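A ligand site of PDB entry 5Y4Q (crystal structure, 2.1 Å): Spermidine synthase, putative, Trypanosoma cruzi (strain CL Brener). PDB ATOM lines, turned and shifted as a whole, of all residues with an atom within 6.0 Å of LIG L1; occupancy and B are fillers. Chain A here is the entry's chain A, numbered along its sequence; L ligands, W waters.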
ATOM      1  N   GLN A  48     -14.788   2.116  25.054  1.00  0.00           N
ATOM      2  CA  GLN A  48     -14.600   0.687  25.434  1.00  0.00           C
ATOM      3  C   GLN A  48     -13.461   0.031  24.692  1.00  0.00           C
ATOM      4  O   GLN A  48     -13.029   0.529  23.654  1.00  0.00           O
ATOM      5  CB  GLN A  48     -15.918  -0.093  25.195  1.00  0.00           C
ATOM      6  CG  GLN A  48     -16.363  -0.151  23.746  1.00  0.00           C
ATOM      7  CD  GLN A  48     -17.868  -0.229  23.579  1.00  0.00           C
ATOM      8  OE1 GLN A  48     -18.561  -0.929  24.345  1.00  0.00           O
ATOM      9  NE2 GLN A  48     -18.394   0.463  22.576  1.00  0.00           N
ATOM     10  N   MET A  65     -16.132 -10.259  17.104  1.00  0.00           N
ATOM     11  CA  MET A  65     -15.970  -8.969  17.784  1.00  0.00           C
ATOM     12  C   MET A  65     -16.266  -9.090  19.275  1.00  0.00           C
ATOM     13  O   MET A  65     -17.354  -9.596  19.669  1.00  0.00           O
ATOM     14  CB  MET A  65     -16.902  -7.926  17.169  1.00  0.00           C
ATOM     15  CG  MET A  65     -16.775  -6.551  17.828  1.00  0.00           C
ATOM     16  SD  MET A  65     -18.075  -5.403  17.365  1.00  0.00           S
ATOM     17  CE  MET A  65     -17.744  -5.309  15.591  1.00  0.00           C
ATOM     18  N   LEU A  67     -16.272  -6.594  22.964  1.00  0.00           N
ATOM     19  CA  LEU A  67     -16.248  -5.274  23.569  1.00  0.00           C
ATOM     20  C   LEU A  67     -15.971  -5.470  25.037  1.00  0.00           C
ATOM     21  O   LEU A  67     -16.681  -6.261  25.692  1.00  0.00           O
ATOM     22  CB  LEU A  67     -17.588  -4.504  23.359  1.00  0.00           C
ATOM     23  CG  LEU A  67     -17.984  -4.098  21.936  1.00  0.00           C
ATOM     24  CD1 LEU A  67     -19.455  -3.716  21.819  1.00  0.00           C
ATOM     25  CD2 LEU A  67     -17.125  -2.933  21.423  1.00  0.00           C
ATOM     26  N   GLN A  72     -19.516 -10.093  21.314  1.00  0.00           N
ATOM     27  CA  GLN A  72     -20.803  -9.473  21.014  1.00  0.00           C
ATOM     28  C   GLN A  72     -21.368  -9.908  19.675  1.00  0.00           C
ATOM     29  O   GLN A  72     -22.575  -9.869  19.472  1.00  0.00           O
ATOM     30  CB  GLN A  72     -20.728  -7.926  21.083  1.00  0.00           C
ATOM     31  CG  GLN A  72     -20.608  -7.326  22.503  1.00  0.00           C
ATOM     32  CD  GLN A  72     -21.637  -7.831  23.526  1.00  0.00           C
ATOM     33  OE1 GLN A  72     -22.774  -8.149  23.204  1.00  0.00           O
ATOM     34  NE2 GLN A  72     -21.213  -7.896  24.787  1.00  0.00           N
ATOM     35  N   VAL A  73     -20.475 -10.311  18.759  1.00  0.00           N
ATOM     36  CA  VAL A  73     -20.863 -10.648  17.401  1.00  0.00           C
ATOM     37  C   VAL A  73     -19.882 -11.683  16.883  1.00  0.00           C
ATOM     38  O   VAL A  73     -18.659 -11.553  17.105  1.00  0.00           O
ATOM     39  CB  VAL A  73     -20.827  -9.424  16.426  1.00  0.00           C
ATOM     40  CG1 VAL A  73     -21.335  -9.838  15.061  1.00  0.00           C
ATOM     41  CG2 VAL A  73     -21.703  -8.295  16.928  1.00  0.00           C
ATOM     42  N   TYR A  81     -29.575 -13.581  17.529  1.00  0.00           N
ATOM     43  CA  TYR A  81     -29.973 -12.441  18.353  1.00  0.00           C
ATOM     44  C   TYR A  81     -30.534 -11.331  17.485  1.00  0.00           C
ATOM     45  O   TYR A  81     -31.487 -10.669  17.889  1.00  0.00           O
ATOM     46  CB  TYR A  81     -28.847 -11.895  19.264  1.00  0.00           C
ATOM     47  CG  TYR A  81     -27.416 -12.156  18.801  1.00  0.00           C
ATOM     48  CD1 TYR A  81     -26.813 -13.424  18.972  1.00  0.00           C
ATOM     49  CD2 TYR A  81     -26.643 -11.122  18.200  1.00  0.00           C
ATOM     50  CE1 TYR A  81     -25.517 -13.663  18.557  1.00  0.00           C
ATOM     51  CE2 TYR A  81     -25.342 -11.349  17.791  1.00  0.00           C
ATOM     52  CZ  TYR A  81     -24.770 -12.610  17.977  1.00  0.00           C
ATOM     53  OH  TYR A  81     -23.476 -12.851  17.586  1.00  0.00           O
ATOM     54  N   HIS A  82     -29.977 -11.196  16.271  1.00  0.00           N
ATOM     55  CA  HIS A  82     -30.441 -10.160  15.355  1.00  0.00           C
ATOM     56  C   HIS A  82     -31.885 -10.348  14.876  1.00  0.00           C
ATOM     57  O   HIS A  82     -32.697  -9.408  14.960  1.00  0.00           O
ATOM     58  CB  HIS A  82     -29.438  -9.929  14.221  1.00  0.00           C
ATOM     59  CG  HIS A  82     -28.153  -9.335  14.729  1.00  0.00           C
ATOM     60  ND1 HIS A  82     -26.933  -9.606  14.170  1.00  0.00           N
ATOM     61  CD2 HIS A  82     -27.906  -8.567  15.811  1.00  0.00           C
ATOM     62  CE1 HIS A  82     -25.988  -8.994  14.863  1.00  0.00           C
ATOM     63  NE2 HIS A  82     -26.555  -8.369  15.873  1.00  0.00           N
ATOM     64  N   ILE A 102     -31.088   1.648  19.759  1.00  0.00           N
ATOM     65  CA  ILE A 102     -30.049   2.176  20.633  1.00  0.00           C
ATOM     66  C   ILE A 102     -28.945   1.117  20.767  1.00  0.00           C
ATOM     67  O   ILE A 102     -29.225  -0.022  21.094  1.00  0.00           O
ATOM     68  CB  ILE A 102     -30.655   2.576  22.016  1.00  0.00           C
ATOM     69  CG1 ILE A 102     -31.555   3.829  21.844  1.00  0.00           C
ATOM     70  CG2 ILE A 102     -29.536   2.815  23.049  1.00  0.00           C
ATOM     71  CD1 ILE A 102     -32.606   4.014  22.948  1.00  0.00           C
ATOM     72  N   GLY A 103     -27.699   1.509  20.500  1.00  0.00           N
ATOM     73  CA  GLY A 103     -26.606   0.567  20.306  1.00  0.00           C
ATOM     74  C   GLY A 103     -26.681   0.012  18.889  1.00  0.00           C
ATOM     75  O   GLY A 103     -27.017   0.738  17.953  1.00  0.00           O
ATOM     76  N   GLY A 104     -26.374  -1.281  18.715  1.00  0.00           N
ATOM     77  CA  GLY A 104     -26.561  -1.931  17.397  1.00  0.00           C
ATOM     78  C   GLY A 104     -25.653  -1.421  16.282  1.00  0.00           C
ATOM     79  O   GLY A 104     -25.977  -1.559  15.086  1.00  0.00           O
ATOM     80  N   GLY A 105     -24.513  -0.840  16.671  1.00  0.00           N
ATOM     81  CA  GLY A 105     -23.570  -0.230  15.761  1.00  0.00           C
ATOM     82  C   GLY A 105     -23.023  -1.143  14.684  1.00  0.00           C
ATOM     83  O   GLY A 105     -22.582  -0.661  13.633  1.00  0.00           O
ATOM     84  N   ASP A 106     -23.055  -2.476  14.928  1.00  0.00           N
ATOM     85  CA  ASP A 106     -22.696  -3.490  13.906  1.00  0.00           C
ATOM     86  C   ASP A 106     -23.683  -3.569  12.728  1.00  0.00           C
ATOM     87  O   ASP A 106     -23.337  -4.055  11.638  1.00  0.00           O
ATOM     88  CB  ASP A 106     -22.553  -4.876  14.582  1.00  0.00           C
ATOM     89  CG  ASP A 106     -23.796  -5.234  15.428  1.00  0.00           C
ATOM     90  OD1 ASP A 106     -24.778  -5.731  14.849  1.00  0.00           O
ATOM     91  OD2 ASP A 106     -23.783  -4.945  16.641  1.00  0.00           O
ATOM     92  N   GLY A 108     -26.607  -5.272  12.618  1.00  0.00           N
ATOM     93  CA  GLY A 108     -27.401  -6.540  12.511  1.00  0.00           C
ATOM     94  C   GLY A 108     -28.880  -6.366  12.738  1.00  0.00           C
ATOM     95  O   GLY A 108     -29.698  -6.784  11.903  1.00  0.00           O
ATOM     96  N   VAL A 109     -29.257  -5.746  13.861  1.00  0.00           N
ATOM     97  CA  VAL A 109     -30.678  -5.481  14.125  1.00  0.00           C
ATOM     98  C   VAL A 109     -31.315  -4.607  13.021  1.00  0.00           C
ATOM     99  O   VAL A 109     -32.406  -4.895  12.537  1.00  0.00           O
ATOM    100  CB  VAL A 109     -30.922  -4.879  15.536  1.00  0.00           C
ATOM    101  CG1 VAL A 109     -32.390  -4.521  15.738  1.00  0.00           C
ATOM    102  CG2 VAL A 109     -30.449  -5.868  16.613  1.00  0.00           C
ATOM    103  N   VAL A 125     -28.691   4.871  16.983  1.00  0.00           N
ATOM    104  CA  VAL A 125     -27.803   5.678  17.786  1.00  0.00           C
ATOM    105  C   VAL A 125     -26.848   4.791  18.606  1.00  0.00           C
ATOM    106  O   VAL A 125     -27.242   4.127  19.583  1.00  0.00           O
ATOM    107  CB  VAL A 125     -28.600   6.586  18.794  1.00  0.00           C
ATOM    108  CG1 VAL A 125     -27.656   7.554  19.488  1.00  0.00           C
ATOM    109  CG2 VAL A 125     -29.706   7.359  18.114  1.00  0.00           C
ATOM    110  N   ASP A 126     -25.578   4.781  18.216  1.00  0.00           N
ATOM    111  CA  ASP A 126     -24.586   4.007  18.973  1.00  0.00           C
ATOM    112  C   ASP A 126     -23.516   4.968  19.467  1.00  0.00           C
ATOM    113  O   ASP A 126     -23.014   5.785  18.708  1.00  0.00           O
ATOM    114  CB  ASP A 126     -23.950   2.897  18.084  1.00  0.00           C
ATOM    115  CG  ASP A 126     -23.111   1.892  18.909  1.00  0.00           C
ATOM    116  OD1 ASP A 126     -22.149   2.291  19.589  1.00  0.00           O
ATOM    117  OD2 ASP A 126     -23.432   0.681  18.885  1.00  0.00           O
ATOM    118  N   ILE A 127     -23.157   4.830  20.749  1.00  0.00           N
ATOM    119  CA  ILE A 127     -22.166   5.699  21.426  1.00  0.00           C
ATOM    120  C   ILE A 127     -20.814   5.651  20.801  1.00  0.00           C
ATOM    121  O   ILE A 127     -20.039   6.615  20.910  1.00  0.00           O
ATOM    122  CB  ILE A 127     -22.104   5.456  22.972  1.00  0.00           C
ATOM    123  CG1 ILE A 127     -21.548   6.692  23.707  1.00  0.00           C
ATOM    124  CG2 ILE A 127     -21.413   4.138  23.327  1.00  0.00           C
ATOM    125  CD1 ILE A 127     -21.726   6.641  25.221  1.00  0.00           C
ATOM    126  N   ASP A 128     -20.498   4.547  20.142  1.00  0.00           N
ATOM    127  CA  ASP A 128     -19.137   4.343  19.752  1.00  0.00           C
ATOM    128  C   ASP A 128     -19.040   4.269  18.241  1.00  0.00           C
ATOM    129  O   ASP A 128     -19.447   3.291  17.622  1.00  0.00           O
ATOM    130  CB  ASP A 128     -18.628   3.099  20.469  1.00  0.00           C
ATOM    131  CG  ASP A 128     -17.125   2.923  20.388  1.00  0.00           C
ATOM    132  OD1 ASP A 128     -16.470   3.399  19.431  1.00  0.00           O
ATOM    133  OD2 ASP A 128     -16.585   2.250  21.299  1.00  0.00           O
ATOM    134  N   VAL A 131     -17.027   1.260  16.525  1.00  0.00           N
ATOM    135  CA  VAL A 131     -17.799   0.025  16.308  1.00  0.00           C
ATOM    136  C   VAL A 131     -18.428  -0.021  14.906  1.00  0.00           C
ATOM    137  O   VAL A 131     -18.277  -1.012  14.203  1.00  0.00           O
ATOM    138  CB  VAL A 131     -18.916  -0.174  17.395  1.00  0.00           C
ATOM    139  CG1 VAL A 131     -19.811  -1.367  17.064  1.00  0.00           C
ATOM    140  CG2 VAL A 131     -18.299  -0.331  18.774  1.00  0.00           C
ATOM    141  N   GLY A 156     -23.644   8.755  19.189  1.00  0.00           N
ATOM    142  CA  GLY A 156     -23.928   9.488  20.412  1.00  0.00           C
ATOM    143  C   GLY A 156     -24.477   8.578  21.488  1.00  0.00           C
ATOM    144  O   GLY A 156     -24.795   7.404  21.221  1.00  0.00           O
ATOM    145  N   ASP A 157     -24.602   9.115  22.686  1.00  0.00           N
ATOM    146  CA  ASP A 157     -25.183   8.395  23.821  1.00  0.00           C
ATOM    147  C   ASP A 157     -26.690   8.256  23.678  1.00  0.00           C
ATOM    148  O   ASP A 157     -27.379   9.265  23.495  1.00  0.00           O
ATOM    149  CB  ASP A 157     -24.822   9.125  25.107  1.00  0.00           C
ATOM    150  CG  ASP A 157     -25.212   8.369  26.385  1.00  0.00           C
ATOM    151  OD1 ASP A 157     -25.775   7.245  26.321  1.00  0.00           O
ATOM    152  OD2 ASP A 157     -24.981   8.931  27.470  1.00  0.00           O
ATOM    153  N   GLY A 158     -27.204   7.022  23.839  1.00  0.00           N
ATOM    154  CA  GLY A 158     -28.630   6.730  23.764  1.00  0.00           C
ATOM    155  C   GLY A 158     -29.440   7.445  24.836  1.00  0.00           C
ATOM    156  O   GLY A 158     -30.598   7.782  24.617  1.00  0.00           O
ATOM    157  N   LEU A 159     -28.834   7.629  26.001  1.00  0.00           N
ATOM    158  CA  LEU A 159     -29.501   8.267  27.152  1.00  0.00           C
ATOM    159  C   LEU A 159     -29.837   9.749  26.859  1.00  0.00           C
ATOM    160  O   LEU A 159     -30.982  10.179  27.043  1.00  0.00           O
ATOM    161  CB  LEU A 159     -28.626   8.136  28.402  1.00  0.00           C
ATOM    162  CG  LEU A 159     -29.169   8.561  29.779  1.00  0.00           C
ATOM    163  CD1 LEU A 159     -30.143   7.547  30.374  1.00  0.00           C
ATOM    164  CD2 LEU A 159     -27.977   8.792  30.723  1.00  0.00           C
ATOM    165  N   ASP A 176     -30.162  -2.534  21.911  1.00  0.00           N
ATOM    166  CA  ASP A 176     -29.223  -3.586  21.560  1.00  0.00           C
ATOM    167  C   ASP A 176     -27.848  -3.207  22.116  1.00  0.00           C
ATOM    168  O   ASP A 176     -26.936  -2.905  21.370  1.00  0.00           O
ATOM    169  CB  ASP A 176     -29.226  -3.775  20.032  1.00  0.00           C
ATOM    170  CG  ASP A 176     -28.285  -4.877  19.570  1.00  0.00           C
ATOM    171  OD1 ASP A 176     -28.077  -5.859  20.310  1.00  0.00           O
ATOM    172  OD2 ASP A 176     -27.770  -4.758  18.429  1.00  0.00           O
ATOM    173  N   THR A 177     -27.703  -3.237  23.431  1.00  0.00           N
ATOM    174  CA  THR A 177     -26.484  -2.730  24.063  1.00  0.00           C
ATOM    175  C   THR A 177     -25.639  -3.837  24.703  1.00  0.00           C
ATOM    176  O   THR A 177     -25.914  -5.026  24.532  1.00  0.00           O
ATOM    177  CB  THR A 177     -26.791  -1.606  25.086  1.00  0.00           C
ATOM    178  OG1 THR A 177     -27.682  -2.111  26.083  1.00  0.00           O
ATOM    179  CG2 THR A 177     -27.410  -0.422  24.388  1.00  0.00           C
ATOM    180  N   THR A 178     -24.612  -3.430  25.447  1.00  0.00           N
ATOM    181  CA  THR A 178     -23.596  -4.343  26.009  1.00  0.00           C
ATOM    182  C   THR A 178     -23.960  -4.940  27.373  1.00  0.00           C
ATOM    183  O   THR A 178     -24.976  -4.590  27.963  1.00  0.00           O
ATOM    184  CB  THR A 178     -22.254  -3.614  26.119  1.00  0.00           C
ATOM    185  OG1 THR A 178     -22.482  -2.229  26.414  1.00  0.00           O
ATOM    186  CG2 THR A 178     -21.487  -3.704  24.799  1.00  0.00           C
ATOM    187  N   GLN A 209     -31.869  -6.255  24.967  1.00  0.00           N
ATOM    188  CA  GLN A 209     -30.982  -7.389  25.242  1.00  0.00           C
ATOM    189  C   GLN A 209     -31.174  -7.690  26.726  1.00  0.00           C
ATOM    190  O   GLN A 209     -30.800  -6.868  27.585  1.00  0.00           O
ATOM    191  CB  GLN A 209     -29.539  -6.988  24.904  1.00  0.00           C
ATOM    192  CG  GLN A 209     -28.464  -8.064  24.998  1.00  0.00           C
ATOM    193  CD  GLN A 209     -27.682  -8.046  26.310  1.00  0.00           C
ATOM    194  OE1 GLN A 209     -26.674  -7.350  26.436  1.00  0.00           O
ATOM    195  NE2 GLN A 209     -28.161  -8.797  27.303  1.00  0.00           N
HETATM  196  C1  LIG L   1     -24.704  -7.282  19.184  1.00  0.00           C
HETATM  197  N1  LIG L   1     -25.522  -6.586  18.170  1.00  0.00           N
HETATM  198  C2  LIG L   1     -25.020  -6.671  20.521  1.00  0.00           C
HETATM  199  C3  LIG L   1     -23.979  -5.682  20.981  1.00  0.00           C
HETATM  200  S1  LIG L   1     -24.090  -4.091  20.107  1.00  0.00           S
HETATM  201  C4  LIG L   1     -22.407  -4.255  19.425  1.00  0.00           C
HETATM  202  C5  LIG L   1     -23.666  -3.100  21.587  1.00  0.00           C
HETATM  203  C6  LIG L   1     -23.549  -1.624  21.260  1.00  0.00           C
HETATM  204  O1  LIG L   1     -24.130  -0.809  22.272  1.00  0.00           O
HETATM  205  C7  LIG L   1     -23.341   0.386  22.270  1.00  0.00           C
HETATM  206  C8  LIG L   1     -21.925  -0.089  22.153  1.00  0.00           C
HETATM  207  O2  LIG L   1     -21.098   0.929  21.605  1.00  0.00           O
HETATM  208  C9  LIG L   1     -22.098  -1.274  21.223  1.00  0.00           C
HETATM  209  O3  LIG L   1     -21.769  -0.973  19.877  1.00  0.00           O
HETATM  210  N2  LIG L   1     -23.627   1.168  23.463  1.00  0.00           N
HETATM  211  C10 LIG L   1     -23.266   0.930  24.758  1.00  0.00           C
HETATM  212  N3  LIG L   1     -23.727   1.873  25.561  1.00  0.00           N
HETATM  213  C11 LIG L   1     -24.412   2.749  24.754  1.00  0.00           C
HETATM  214  C12 LIG L   1     -25.100   3.928  25.020  1.00  0.00           C
HETATM  215  N4  LIG L   1     -25.227   4.464  26.313  1.00  0.00           N
HETATM  216  C13 LIG L   1     -24.358   2.318  23.436  1.00  0.00           C
HETATM  217  N5  LIG L   1     -24.905   2.913  22.370  1.00  0.00           N
HETATM  218  C14 LIG L   1     -25.540   4.020  22.758  1.00  0.00           C
HETATM  219  N6  LIG L   1     -25.667   4.555  23.980  1.00  0.00           N
HETATM  220  C1  LG2 L   2     -19.119 -18.106  20.626  1.00  0.00           C
HETATM  221  C2  LG2 L   2     -18.048 -18.220  21.486  1.00  0.00           C
HETATM  222  C3  LG2 L   2     -20.166 -17.232  20.868  1.00  0.00           C
HETATM  223  C4  LG2 L   2     -18.027 -17.446  22.613  1.00  0.00           C
HETATM  224  C5  LG2 L   2     -24.524 -14.520  21.683  1.00  0.00           C
HETATM  225  C6  LG2 L   2     -22.918 -12.753  21.933  1.00  0.00           C
HETATM  226  C7  LG2 L   2     -25.558 -13.613  21.731  1.00  0.00           C
HETATM  227  C8  LG2 L   2     -23.956 -11.832  21.936  1.00  0.00           C
HETATM  228  C9  LG2 L   2     -20.994 -14.821  23.535  1.00  0.00           C
HETATM  229  C10 LG2 L   2     -19.897 -14.991  24.327  1.00  0.00           C
HETATM  230  C11 LG2 L   2     -20.140 -16.446  22.000  1.00  0.00           C
HETATM  231  C12 LG2 L   2     -19.056 -16.566  22.876  1.00  0.00           C
HETATM  232  C13 LG2 L   2     -23.219 -14.102  21.842  1.00  0.00           C
HETATM  233  C14 LG2 L   2     -21.117 -15.520  22.349  1.00  0.00           C
HETATM  234  C15 LG2 L   2     -25.280 -12.263  21.841  1.00  0.00           C
HETATM  235  C16 LG2 L   2     -26.108 -10.065  22.070  1.00  0.00           C
HETATM  236  N1  LG2 L   2     -18.942 -15.857  23.997  1.00  0.00           N
HETATM  237  N2  LG2 L   2     -22.342 -15.187  21.841  1.00  0.00           N
HETATM  238  O1  LG2 L   2     -26.413 -11.449  21.824  1.00  0.00           O
HETATM  239  O   HOH W   1     -27.194  -4.865  15.815  1.00  0.00           O
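Water W1 lies within hydrogen-bond range of the side-chain carboxylate (OD2) of Asp 176 (2.7 Å), the side-chain carboxylate (OD1) of Asp 106 (2.7 Å), the backbone NH (N) of Val 109 (3.0 Å), the backbone NH (N) of Gly 108 (3.3 Å) and a nitrogen (N1) of LIG L1 (3.4 Å).
O of Asp 126 lies within hydrogen-bond range of N of Gly 156 (3.1 Å). OD1 of Asp 157 is in hydrogen-bond range of N of Leu 159 (3.1 Å). A ring nitrogen (NE2) of His 82 lies within hydrogen-bond range of the side-chain carboxylate of Asp 106, at 3.3 Å. The backbone NH (N) of Gly 108 is in hydrogen-bond range of the side-chain carboxylate (OD1) of Asp 106 (2.9 Å). O of Asp 176 is in hydrogen-bond range of N of Gly 104 (3.2 Å). O of Ile 102 lies within hydrogen-bond range of N of Asp 176. OD2 of Asp 128 sits at hydrogen-bond distance from NE2 of Gln 48 (2.8 Å). The backbone carbonyl oxygen of Val 73 sits at hydrogen-bond distance from the backbone NH of Met 65, at 2.8 Å.
An oxygen (O3) of LIG L1 lies within hydrogen-bond range of the side-chain carboxylate (OD2) of Asp 126 (2.5 Å). The side-chain carboxylate (OD1) of Asp 157 is in hydrogen-bond range of a nitrogen (N4) of LIG L1. The side-chain carboxylate (OD2) of Asp 106 is in salt-bridge range of a nitrogen (N1) of LIG L1, 2.8 Å away. O of Asp 176 lies close to S1 of LIG L1 (3.3 Å). N1 of LIG L1 is in salt-bridge range of OD2 of Asp 176, at 2.9 Å. N of Gly 158 is in hydrogen-bond range of N6 of LIG L1, 2.9 Å away. The side-chain amide nitrogen (NE2) of Gln 48 sits at hydrogen-bond distance from an oxygen (O2) of LIG L1 (2.9 Å). N of Ile 127 sits at hydrogen-bond distance from N5 of LIG L1 (3.1 Å). A nitrogen (N1) of LIG L1 is in hydrogen-bond range of a ring nitrogen (NE2) of His 82.
Leu 67 touches LIG L1. Gln 72 touches LIG L1 (O to C1, 3.4 Å). CG2 of Val 73 touches C1 of LIG L1, at 3.9 Å. CA of Gly 103 touches O1 of LIG L1, 3.4 Å away. Gly 104 touches LIG L1. Val 125 touches LIG L1. Asp 128 touches LIG L1. Val 131 touches LIG L1 (CG1 to O3, 3.4 Å). Gly 156 touches LIG L1. Thr 177 touches LIG L1. Thr 178 touches LIG L1 (OG1 to C10, 3.7 Å). The nearest printed residue that does not touch LIG L1 is Ile 102 (4.2 Å).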
